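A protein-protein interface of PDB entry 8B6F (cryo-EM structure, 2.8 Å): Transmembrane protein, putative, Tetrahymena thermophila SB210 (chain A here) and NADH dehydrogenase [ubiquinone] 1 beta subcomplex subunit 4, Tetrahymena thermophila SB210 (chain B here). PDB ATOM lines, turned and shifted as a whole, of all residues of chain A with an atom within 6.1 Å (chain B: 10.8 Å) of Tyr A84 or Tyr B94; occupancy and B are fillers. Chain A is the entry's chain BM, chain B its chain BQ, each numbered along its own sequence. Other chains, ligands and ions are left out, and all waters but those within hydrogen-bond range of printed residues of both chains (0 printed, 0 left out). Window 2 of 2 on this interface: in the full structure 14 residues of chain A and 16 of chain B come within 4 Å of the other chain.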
ATOM      1  N   ASP A  77     -36.290  -6.290  -2.468  1.00  0.00           N
ATOM      2  CA  ASP A  77     -35.305  -5.367  -3.017  1.00  0.00           C
ATOM      3  C   ASP A  77     -35.913  -3.991  -3.249  1.00  0.00           C
ATOM      4  O   ASP A  77     -35.278  -2.968  -2.976  1.00  0.00           O
ATOM      5  CB  ASP A  77     -34.735  -5.920  -4.320  1.00  0.00           C
ATOM      6  CG  ASP A  77     -33.839  -4.927  -5.024  1.00  0.00           C
ATOM      7  OD1 ASP A  77     -32.704  -4.709  -4.553  1.00  0.00           O
ATOM      8  OD2 ASP A  77     -34.273  -4.357  -6.047  1.00  0.00           O
ATOM      9  N   GLY A  80     -36.197  -2.220  -0.063  1.00  0.00           N
ATOM     10  CA  GLY A  80     -34.880  -1.825   0.401  1.00  0.00           C
ATOM     11  C   GLY A  80     -34.232  -0.721  -0.408  1.00  0.00           C
ATOM     12  O   GLY A  80     -33.282  -0.095   0.074  1.00  0.00           O
ATOM     13  N   ARG A  81     -34.714  -0.469  -1.627  1.00  0.00           N
ATOM     14  CA  ARG A  81     -34.144   0.578  -2.468  1.00  0.00           C
ATOM     15  C   ARG A  81     -34.443   1.982  -1.963  1.00  0.00           C
ATOM     16  O   ARG A  81     -34.037   2.948  -2.617  1.00  0.00           O
ATOM     17  CB  ARG A  81     -34.655   0.440  -3.903  1.00  0.00           C
ATOM     18  CG  ARG A  81     -33.919  -0.601  -4.721  1.00  0.00           C
ATOM     19  CD  ARG A  81     -34.476  -0.696  -6.128  1.00  0.00           C
ATOM     20  NE  ARG A  81     -34.121   0.462  -6.937  1.00  0.00           N
ATOM     21  CZ  ARG A  81     -34.451   0.615  -8.212  1.00  0.00           C
ATOM     22  NH1 ARG A  81     -35.154  -0.299  -8.859  1.00  0.00           N
ATOM     23  NH2 ARG A  81     -34.068   1.714  -8.854  1.00  0.00           N
ATOM     24  N   GLU A  82     -35.138   2.129  -0.833  1.00  0.00           N
ATOM     25  CA  GLU A  82     -35.399   3.458  -0.295  1.00  0.00           C
ATOM     26  C   GLU A  82     -34.116   4.196   0.059  1.00  0.00           C
ATOM     27  O   GLU A  82     -34.135   5.424   0.190  1.00  0.00           O
ATOM     28  CB  GLU A  82     -36.290   3.357   0.944  1.00  0.00           C
ATOM     29  CG  GLU A  82     -37.639   2.698   0.692  1.00  0.00           C
ATOM     30  CD  GLU A  82     -38.542   3.524  -0.203  1.00  0.00           C
ATOM     31  OE1 GLU A  82     -38.157   4.655  -0.559  1.00  0.00           O
ATOM     32  OE2 GLU A  82     -39.640   3.042  -0.548  1.00  0.00           O
ATOM     33  N   LYS A  83     -33.004   3.477   0.219  1.00  0.00           N
ATOM     34  CA  LYS A  83     -31.743   4.128   0.558  1.00  0.00           C
ATOM     35  C   LYS A  83     -31.279   5.054  -0.559  1.00  0.00           C
ATOM     36  O   LYS A  83     -30.702   6.116  -0.297  1.00  0.00           O
ATOM     37  CB  LYS A  83     -30.676   3.075   0.858  1.00  0.00           C
ATOM     38  CG  LYS A  83     -30.468   2.060  -0.262  1.00  0.00           C
ATOM     39  CD  LYS A  83     -29.294   1.135   0.020  1.00  0.00           C
ATOM     40  CE  LYS A  83     -27.964   1.863  -0.120  1.00  0.00           C
ATOM     41  NZ  LYS A  83     -26.803   0.951   0.075  1.00  0.00           N
ATOM     42  N   TYR A  84     -31.518   4.671  -1.810  1.00  0.00           N
ATOM     43  CA  TYR A  84     -31.022   5.444  -2.936  1.00  0.00           C
ATOM     44  C   TYR A  84     -31.751   6.782  -3.035  1.00  0.00           C
ATOM     45  O   TYR A  84     -32.760   7.029  -2.369  1.00  0.00           O
ATOM     46  CB  TYR A  84     -31.190   4.660  -4.237  1.00  0.00           C
ATOM     47  CG  TYR A  84     -30.466   3.335  -4.248  1.00  0.00           C
ATOM     48  CD1 TYR A  84     -29.089   3.275  -4.420  1.00  0.00           C
ATOM     49  CD2 TYR A  84     -31.161   2.143  -4.096  1.00  0.00           C
ATOM     50  CE1 TYR A  84     -28.425   2.063  -4.435  1.00  0.00           C
ATOM     51  CE2 TYR A  84     -30.507   0.928  -4.110  1.00  0.00           C
ATOM     52  CZ  TYR A  84     -29.139   0.894  -4.279  1.00  0.00           C
ATOM     53  OH  TYR A  84     -28.488  -0.316  -4.293  1.00  0.00           O
ATOM     54  N   ALA A  85     -31.218   7.657  -3.884  1.00  0.00           N
ATOM     55  CA  ALA A  85     -31.828   8.956  -4.104  1.00  0.00           C
ATOM     56  C   ALA A  85     -33.227   8.787  -4.693  1.00  0.00           C
ATOM     57  O   ALA A  85     -33.630   7.701  -5.112  1.00  0.00           O
ATOM     58  CB  ALA A  85     -30.959   9.804  -5.030  1.00  0.00           C
ATOM     59  N   GLN A  86     -33.972   9.892  -4.723  1.00  0.00           N
ATOM     60  CA  GLN A  86     -35.353   9.835  -5.200  1.00  0.00           C
ATOM     61  C   GLN A  86     -35.467   9.273  -6.608  1.00  0.00           C
ATOM     62  O   GLN A  86     -36.294   8.370  -6.822  1.00  0.00           O
ATOM     63  CB  GLN A  86     -35.978  11.232  -5.115  1.00  0.00           C
ATOM     64  CG  GLN A  86     -37.405  11.307  -5.642  1.00  0.00           C
ATOM     65  CD  GLN A  86     -38.341  10.350  -4.935  1.00  0.00           C
ATOM     66  OE1 GLN A  86     -38.079   9.922  -3.814  1.00  0.00           O
ATOM     67  NE2 GLN A  86     -39.442  10.008  -5.592  1.00  0.00           N
ATOM     68  N   TYR A  88     -33.836   7.140  -8.167  1.00  0.00           N
ATOM     69  CA  TYR A  88     -33.421   5.748  -8.274  1.00  0.00           C
ATOM     70  C   TYR A  88     -34.158   4.834  -7.304  1.00  0.00           C
ATOM     71  O   TYR A  88     -33.788   3.664  -7.169  1.00  0.00           O
ATOM     72  CB  TYR A  88     -31.912   5.641  -8.060  1.00  0.00           C
ATOM     73  CG  TYR A  88     -31.149   6.613  -8.922  1.00  0.00           C
ATOM     74  CD1 TYR A  88     -31.078   6.437 -10.295  1.00  0.00           C
ATOM     75  CD2 TYR A  88     -30.523   7.719  -8.368  1.00  0.00           C
ATOM     76  CE1 TYR A  88     -30.394   7.326 -11.094  1.00  0.00           C
ATOM     77  CE2 TYR A  88     -29.835   8.617  -9.158  1.00  0.00           C
ATOM     78  CZ  TYR A  88     -29.779   8.415 -10.521  1.00  0.00           C
ATOM     79  OH  TYR A  88     -29.097   9.300 -11.321  1.00  0.00           O
ATOM     80  N   LYS A  89     -35.188   5.333  -6.628  1.00  0.00           N
ATOM     81  CA  LYS A  89     -36.016   4.464  -5.812  1.00  0.00           C
ATOM     82  C   LYS A  89     -36.849   3.553  -6.709  1.00  0.00           C
ATOM     83  O   LYS A  89     -37.045   3.814  -7.898  1.00  0.00           O
ATOM     84  CB  LYS A  89     -36.928   5.284  -4.901  1.00  0.00           C
ATOM     85  CG  LYS A  89     -36.183   6.153  -3.904  1.00  0.00           C
ATOM     86  CD  LYS A  89     -37.144   6.857  -2.962  1.00  0.00           C
ATOM     87  CE  LYS A  89     -36.405   7.722  -1.959  1.00  0.00           C
ATOM     88  NZ  LYS A  89     -35.500   6.925  -1.090  1.00  0.00           N
ATOM     89  N   ILE B  86     -24.523 -18.667  -7.586  1.00  0.00           N
ATOM     90  CA  ILE B  86     -25.764 -17.898  -7.627  1.00  0.00           C
ATOM     91  C   ILE B  86     -25.650 -16.649  -6.763  1.00  0.00           C
ATOM     92  O   ILE B  86     -26.059 -15.556  -7.171  1.00  0.00           O
ATOM     93  CB  ILE B  86     -26.949 -18.781  -7.195  1.00  0.00           C
ATOM     94  CG1 ILE B  86     -27.160 -19.906  -8.210  1.00  0.00           C
ATOM     95  CG2 ILE B  86     -28.223 -17.951  -7.060  1.00  0.00           C
ATOM     96  CD1 ILE B  86     -28.101 -20.983  -7.737  1.00  0.00           C
ATOM     97  N   ILE B  87     -25.100 -16.788  -5.555  1.00  0.00           N
ATOM     98  CA  ILE B  87     -24.962 -15.631  -4.674  1.00  0.00           C
ATOM     99  C   ILE B  87     -24.055 -14.588  -5.313  1.00  0.00           C
ATOM    100  O   ILE B  87     -24.350 -13.388  -5.287  1.00  0.00           O
ATOM    101  CB  ILE B  87     -24.444 -16.068  -3.291  1.00  0.00           C
ATOM    102  CG1 ILE B  87     -25.492 -16.941  -2.595  1.00  0.00           C
ATOM    103  CG2 ILE B  87     -24.111 -14.852  -2.430  1.00  0.00           C
ATOM    104  CD1 ILE B  87     -25.013 -17.569  -1.302  1.00  0.00           C
ATOM    105  N   GLY B  88     -22.935 -15.028  -5.885  1.00  0.00           N
ATOM    106  CA  GLY B  88     -22.045 -14.092  -6.550  1.00  0.00           C
ATOM    107  C   GLY B  88     -22.707 -13.390  -7.720  1.00  0.00           C
ATOM    108  O   GLY B  88     -22.516 -12.190  -7.924  1.00  0.00           O
ATOM    109  N   GLY B  89     -23.495 -14.128  -8.503  1.00  0.00           N
ATOM    110  CA  GLY B  89     -24.190 -13.507  -9.618  1.00  0.00           C
ATOM    111  C   GLY B  89     -25.178 -12.448  -9.172  1.00  0.00           C
ATOM    112  O   GLY B  89     -25.262 -11.375  -9.772  1.00  0.00           O
ATOM    113  N   PHE B  90     -25.945 -12.736  -8.119  1.00  0.00           N
ATOM    114  CA  PHE B  90     -26.876 -11.738  -7.600  1.00  0.00           C
ATOM    115  C   PHE B  90     -26.135 -10.515  -7.079  1.00  0.00           C
ATOM    116  O   PHE B  90     -26.568  -9.379  -7.298  1.00  0.00           O
ATOM    117  CB  PHE B  90     -27.750 -12.347  -6.503  1.00  0.00           C
ATOM    118  CG  PHE B  90     -28.770 -13.338  -7.004  1.00  0.00           C
ATOM    119  CD1 PHE B  90     -28.947 -13.567  -8.361  1.00  0.00           C
ATOM    120  CD2 PHE B  90     -29.563 -14.033  -6.107  1.00  0.00           C
ATOM    121  CE1 PHE B  90     -29.888 -14.473  -8.810  1.00  0.00           C
ATOM    122  CE2 PHE B  90     -30.506 -14.941  -6.549  1.00  0.00           C
ATOM    123  CZ  PHE B  90     -30.668 -15.161  -7.903  1.00  0.00           C
ATOM    124  N   THR B  91     -25.019 -10.724  -6.378  1.00  0.00           N
ATOM    125  CA  THR B  91     -24.235  -9.593  -5.897  1.00  0.00           C
ATOM    126  C   THR B  91     -23.726  -8.747  -7.056  1.00  0.00           C
ATOM    127  O   THR B  91     -23.758  -7.513  -6.993  1.00  0.00           O
ATOM    128  CB  THR B  91     -23.064 -10.085  -5.045  1.00  0.00           C
ATOM    129  OG1 THR B  91     -23.558 -10.865  -3.949  1.00  0.00           O
ATOM    130  CG2 THR B  91     -22.260  -8.911  -4.501  1.00  0.00           C
ATOM    131  N   TYR B  92     -23.252  -9.391  -8.123  1.00  0.00           N
ATOM    132  CA  TYR B  92     -22.750  -8.638  -9.267  1.00  0.00           C
ATOM    133  C   TYR B  92     -23.864  -7.873  -9.965  1.00  0.00           C
ATOM    134  O   TYR B  92     -23.651  -6.755 -10.446  1.00  0.00           O
ATOM    135  CB  TYR B  92     -22.060  -9.574 -10.255  1.00  0.00           C
ATOM    136  CG  TYR B  92     -21.444  -8.840 -11.419  1.00  0.00           C
ATOM    137  CD1 TYR B  92     -20.183  -8.270 -11.322  1.00  0.00           C
ATOM    138  CD2 TYR B  92     -22.133  -8.711 -12.617  1.00  0.00           C
ATOM    139  CE1 TYR B  92     -19.626  -7.594 -12.385  1.00  0.00           C
ATOM    140  CE2 TYR B  92     -21.585  -8.039 -13.685  1.00  0.00           C
ATOM    141  CZ  TYR B  92     -20.330  -7.484 -13.565  1.00  0.00           C
ATOM    142  OH  TYR B  92     -19.783  -6.812 -14.630  1.00  0.00           O
ATOM    143  N   CYS B  93     -25.057  -8.458 -10.034  1.00  0.00           N
ATOM    144  CA  CYS B  93     -26.190  -7.741 -10.602  1.00  0.00           C
ATOM    145  C   CYS B  93     -26.528  -6.516  -9.766  1.00  0.00           C
ATOM    146  O   CYS B  93     -26.838  -5.450 -10.308  1.00  0.00           O
ATOM    147  CB  CYS B  93     -27.378  -8.688 -10.722  1.00  0.00           C
ATOM    148  SG  CYS B  93     -27.099  -9.896 -12.033  1.00  0.00           S
ATOM    149  N   TYR B  94     -26.480  -6.651  -8.440  1.00  0.00           N
ATOM    150  CA  TYR B  94     -26.687  -5.499  -7.572  1.00  0.00           C
ATOM    151  C   TYR B  94     -25.657  -4.416  -7.866  1.00  0.00           C
ATOM    152  O   TYR B  94     -25.991  -3.230  -7.963  1.00  0.00           O
ATOM    153  CB  TYR B  94     -26.613  -5.948  -6.112  1.00  0.00           C
ATOM    154  CG  TYR B  94     -27.047  -4.914  -5.103  1.00  0.00           C
ATOM    155  CD1 TYR B  94     -26.185  -3.901  -4.705  1.00  0.00           C
ATOM    156  CD2 TYR B  94     -28.306  -4.971  -4.522  1.00  0.00           C
ATOM    157  CE1 TYR B  94     -26.572  -2.960  -3.772  1.00  0.00           C
ATOM    158  CE2 TYR B  94     -28.704  -4.034  -3.588  1.00  0.00           C
ATOM    159  CZ  TYR B  94     -27.832  -3.031  -3.217  1.00  0.00           C
ATOM    160  OH  TYR B  94     -28.220  -2.095  -2.287  1.00  0.00           O
ATOM    161  N   HIS B  95     -24.388  -4.811  -8.002  1.00  0.00           N
ATOM    162  CA  HIS B  95     -23.333  -3.852  -8.312  1.00  0.00           C
ATOM    163  C   HIS B  95     -23.559  -3.200  -9.670  1.00  0.00           C
ATOM    164  O   HIS B  95     -23.323  -1.999  -9.840  1.00  0.00           O
ATOM    165  CB  HIS B  95     -21.970  -4.542  -8.278  1.00  0.00           C
ATOM    166  CG  HIS B  95     -20.845  -3.674  -8.749  1.00  0.00           C
ATOM    167  ND1 HIS B  95     -20.242  -3.839  -9.978  1.00  0.00           N
ATOM    168  CD2 HIS B  95     -20.216  -2.633  -8.158  1.00  0.00           C
ATOM    169  CE1 HIS B  95     -19.291  -2.934 -10.124  1.00  0.00           C
ATOM    170  NE2 HIS B  95     -19.253  -2.191  -9.033  1.00  0.00           N
ATOM    171  N   MET B  96     -24.016  -3.982 -10.649  1.00  0.00           N
ATOM    172  CA  MET B  96     -24.279  -3.438 -11.976  1.00  0.00           C
ATOM    173  C   MET B  96     -25.388  -2.395 -11.938  1.00  0.00           C
ATOM    174  O   MET B  96     -25.301  -1.363 -12.613  1.00  0.00           O
ATOM    175  CB  MET B  96     -24.638  -4.575 -12.933  1.00  0.00           C
ATOM    176  CG  MET B  96     -24.927  -4.127 -14.353  1.00  0.00           C
ATOM    177  SD  MET B  96     -24.968  -5.509 -15.511  1.00  0.00           S
ATOM    178  CE  MET B  96     -26.185  -6.571 -14.739  1.00  0.00           C
ATOM    179  N   ARG B  97     -26.440  -2.644 -11.159  1.00  0.00           N
ATOM    180  CA  ARG B  97     -27.495  -1.646 -11.018  1.00  0.00           C
ATOM    181  C   ARG B  97     -26.965  -0.377 -10.363  1.00  0.00           C
ATOM    182  O   ARG B  97     -27.316   0.735 -10.775  1.00  0.00           O
ATOM    183  CB  ARG B  97     -28.659  -2.218 -10.217  1.00  0.00           C
ATOM    184  CG  ARG B  97     -29.858  -1.294 -10.163  1.00  0.00           C
ATOM    185  CD  ARG B  97     -31.023  -1.950  -9.462  1.00  0.00           C
ATOM    186  NE  ARG B  97     -30.706  -2.283  -8.080  1.00  0.00           N
ATOM    187  CZ  ARG B  97     -31.533  -2.912  -7.258  1.00  0.00           C
ATOM    188  NH1 ARG B  97     -32.734  -3.298  -7.652  1.00  0.00           N
ATOM    189  NH2 ARG B  97     -31.142  -3.167  -6.013  1.00  0.00           N
ATOM    190  N   GLU B  98     -26.116  -0.520  -9.345  1.00  0.00           N
ATOM    191  CA  GLU B  98     -25.497   0.651  -8.732  1.00  0.00           C
ATOM    192  C   GLU B  98     -24.671   1.418  -9.754  1.00  0.00           C
ATOM    193  O   GLU B  98     -24.686   2.652  -9.780  1.00  0.00           O
ATOM    194  CB  GLU B  98     -24.628   0.227  -7.546  1.00  0.00           C
ATOM    195  CG  GLU B  98     -23.834   1.361  -6.909  1.00  0.00           C
ATOM    196  CD  GLU B  98     -24.716   2.482  -6.396  1.00  0.00           C
ATOM    197  OE1 GLU B  98     -25.924   2.243  -6.193  1.00  0.00           O
ATOM    198  OE2 GLU B  98     -24.203   3.604  -6.197  1.00  0.00           O
ATOM    199  N   THR B  99     -23.944   0.696 -10.607  1.00  0.00           N
ATOM    200  CA  THR B  99     -23.173   1.346 -11.660  1.00  0.00           C
ATOM    201  C   THR B  99     -24.079   2.129 -12.599  1.00  0.00           C
ATOM    202  O   THR B  99     -23.741   3.244 -13.014  1.00  0.00           O
ATOM    203  CB  THR B  99     -22.369   0.298 -12.433  1.00  0.00           C
ATOM    204  OG1 THR B  99     -21.145   0.018 -11.742  1.00  0.00           O
ATOM    205  CG2 THR B  99     -22.074   0.762 -13.851  1.00  0.00           C
ATOM    206  N   ARG B 100     -25.232   1.561 -12.949  1.00  0.00           N
ATOM    207  CA  ARG B 100     -26.181   2.273 -13.796  1.00  0.00           C
ATOM    208  C   ARG B 100     -26.666   3.549 -13.121  1.00  0.00           C
ATOM    209  O   ARG B 100     -26.799   4.592 -13.772  1.00  0.00           O
ATOM    210  CB  ARG B 100     -27.358   1.366 -14.144  1.00  0.00           C
ATOM    211  CG  ARG B 100     -28.269   1.947 -15.204  1.00  0.00           C
ATOM    212  CD  ARG B 100     -29.548   1.147 -15.335  1.00  0.00           C
ATOM    213  NE  ARG B 100     -30.473   1.398 -14.236  1.00  0.00           N
ATOM    214  CZ  ARG B 100     -31.144   2.529 -14.060  1.00  0.00           C
ATOM    215  NH1 ARG B 100     -30.980   3.563 -14.868  1.00  0.00           N
ATOM    216  NH2 ARG B 100     -31.997   2.627 -13.046  1.00  0.00           N
ATOM    217  N   PHE B 101     -26.943   3.487 -11.818  1.00  0.00           N
ATOM    218  CA  PHE B 101     -27.317   4.694 -11.089  1.00  0.00           C
ATOM    219  C   PHE B 101     -26.228   5.753 -11.198  1.00  0.00           C
ATOM    220  O   PHE B 101     -26.517   6.929 -11.444  1.00  0.00           O
ATOM    221  CB  PHE B 101     -27.578   4.366  -9.617  1.00  0.00           C
ATOM    222  CG  PHE B 101     -28.759   3.464  -9.382  1.00  0.00           C
ATOM    223  CD1 PHE B 101     -29.761   3.327 -10.330  1.00  0.00           C
ATOM    224  CD2 PHE B 101     -28.868   2.760  -8.195  1.00  0.00           C
ATOM    225  CE1 PHE B 101     -30.839   2.499 -10.098  1.00  0.00           C
ATOM    226  CE2 PHE B 101     -29.943   1.933  -7.960  1.00  0.00           C
ATOM    227  CZ  PHE B 101     -30.930   1.803  -8.911  1.00  0.00           C
ATOM    228  N   GLN B 102     -24.967   5.354 -11.025  1.00  0.00           N
ATOM    229  CA  GLN B 102     -23.869   6.313 -11.101  1.00  0.00           C
ATOM    230  C   GLN B 102     -23.783   6.943 -12.484  1.00  0.00           C
ATOM    231  O   GLN B 102     -23.578   8.155 -12.611  1.00  0.00           O
ATOM    232  CB  GLN B 102     -22.553   5.627 -10.739  1.00  0.00           C
ATOM    233  CG  GLN B 102     -22.510   5.102  -9.315  1.00  0.00           C
ATOM    234  CD  GLN B 102     -21.288   4.250  -9.049  1.00  0.00           C
ATOM    235  OE1 GLN B 102     -20.360   4.207  -9.854  1.00  0.00           O
ATOM    236  NE2 GLN B 102     -21.285   3.560  -7.915  1.00  0.00           N
ATOM    237  N   ASP B 104     -26.231   7.338 -14.623  1.00  0.00           N
ATOM    238  CA  ASP B 104     -27.356   8.257 -14.753  1.00  0.00           C
ATOM    239  C   ASP B 104     -27.069   9.575 -14.047  1.00  0.00           C
ATOM    240  O   ASP B 104     -27.368  10.649 -14.580  1.00  0.00           O
ATOM    241  CB  ASP B 104     -28.628   7.619 -14.194  1.00  0.00           C
ATOM    242  CG  ASP B 104     -29.233   6.595 -15.137  1.00  0.00           C
ATOM    243  OD1 ASP B 104     -29.150   6.794 -16.366  1.00  0.00           O
ATOM    244  OD2 ASP B 104     -29.798   5.596 -14.648  1.00  0.00           O
ATOM    245  N   ASP B 105     -26.489   9.515 -12.846  1.00  0.00           N
ATOM    246  CA  ASP B 105     -26.147  10.743 -12.135  1.00  0.00           C
ATOM    247  C   ASP B 105     -25.152  11.576 -12.928  1.00  0.00           C
ATOM    248  O   ASP B 105     -25.301  12.799 -13.038  1.00  0.00           O
ATOM    249  CB  ASP B 105     -25.567  10.415 -10.758  1.00  0.00           C
ATOM    250  CG  ASP B 105     -26.624  10.002  -9.758  1.00  0.00           C
ATOM    251  OD1 ASP B 105     -27.730  10.579  -9.791  1.00  0.00           O
ATOM    252  OD2 ASP B 105     -26.349   9.104  -8.934  1.00  0.00           O
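NH1 of Arg B97 is in salt-bridge range of OD2 of Asp A77, 2.5 Å away. OH of Tyr A84 sits at hydrogen-bond distance from OH of Tyr B94 (2.7 Å). OH of Tyr A88 is in hydrogen-bond range of OD1 of Asp B105 (2.4 Å).
Arg A81 touches Arg B97. NH2 of Arg A81 touches CZ of Phe B101 (3.1 Å). Tyr A84 touches Glu B98 (CE1 to OE1, 3.1 Å). Phe B101 touches Tyr A84. Tyr A88 touches Phe B101 (CD1 to CD1, 3.4 Å). CB of Asp B104 touches OH of Tyr A88, 3.4 Å away.
NH2 of Arg A81 is in hydrogen-bond range of O of Tyr A88, at 2.6 Å. The backbone carbonyl oxygen of Tyr A84 is in hydrogen-bond range of the side-chain amino group of Lys A89 (3.0 Å). NE2 of Gln B102 is in hydrogen-bond range of OE2 of Glu B98, at 3.4 Å.
Of the 10 printed residues of chain A, 4 touch a printed residue of chain B. Hydrophobic or aromatic side chains of chain A within 4 Å of the printed part of chain B: Tyr A84 and Tyr A88. Of the 19 printed residues of chain B, 6 touch a printed residue of chain A. Printed residues of chain B that touch a printed residue of chain A: Tyr B94, Arg B97, Glu B98, Phe B101, Asp B104 and Asp B105. Among the printed residues, 9 pairs touch across the chains. Among the printed residues, Asp or Glu carboxylates within 4 Å of a Lys or Arg side-chain nitrogen of the other chain: Asp A77 with Arg B97.
Of the printed residues of chain B, Asp A77 touches Arg B97. No residue of chain B comes within 4 Å of Lys A83. Tyr A84 touches three residues of chain B. Of the printed residues of chain B, Tyr A88 touches Phe B101, Asp B104 and Asp B105. Of chain A, only Tyr A84 comes within 4 Å of Tyr B94. Of the printed residues of chain A, Arg B97 touches Asp A77 and Arg A81. Arg B100 touches none of the printed residues of chain A. Of the printed residues of chain A, Asp B104 touches Tyr A88 (3.4 Å). Of the printed residues of chain A, Asp B105 touches Tyr A88.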
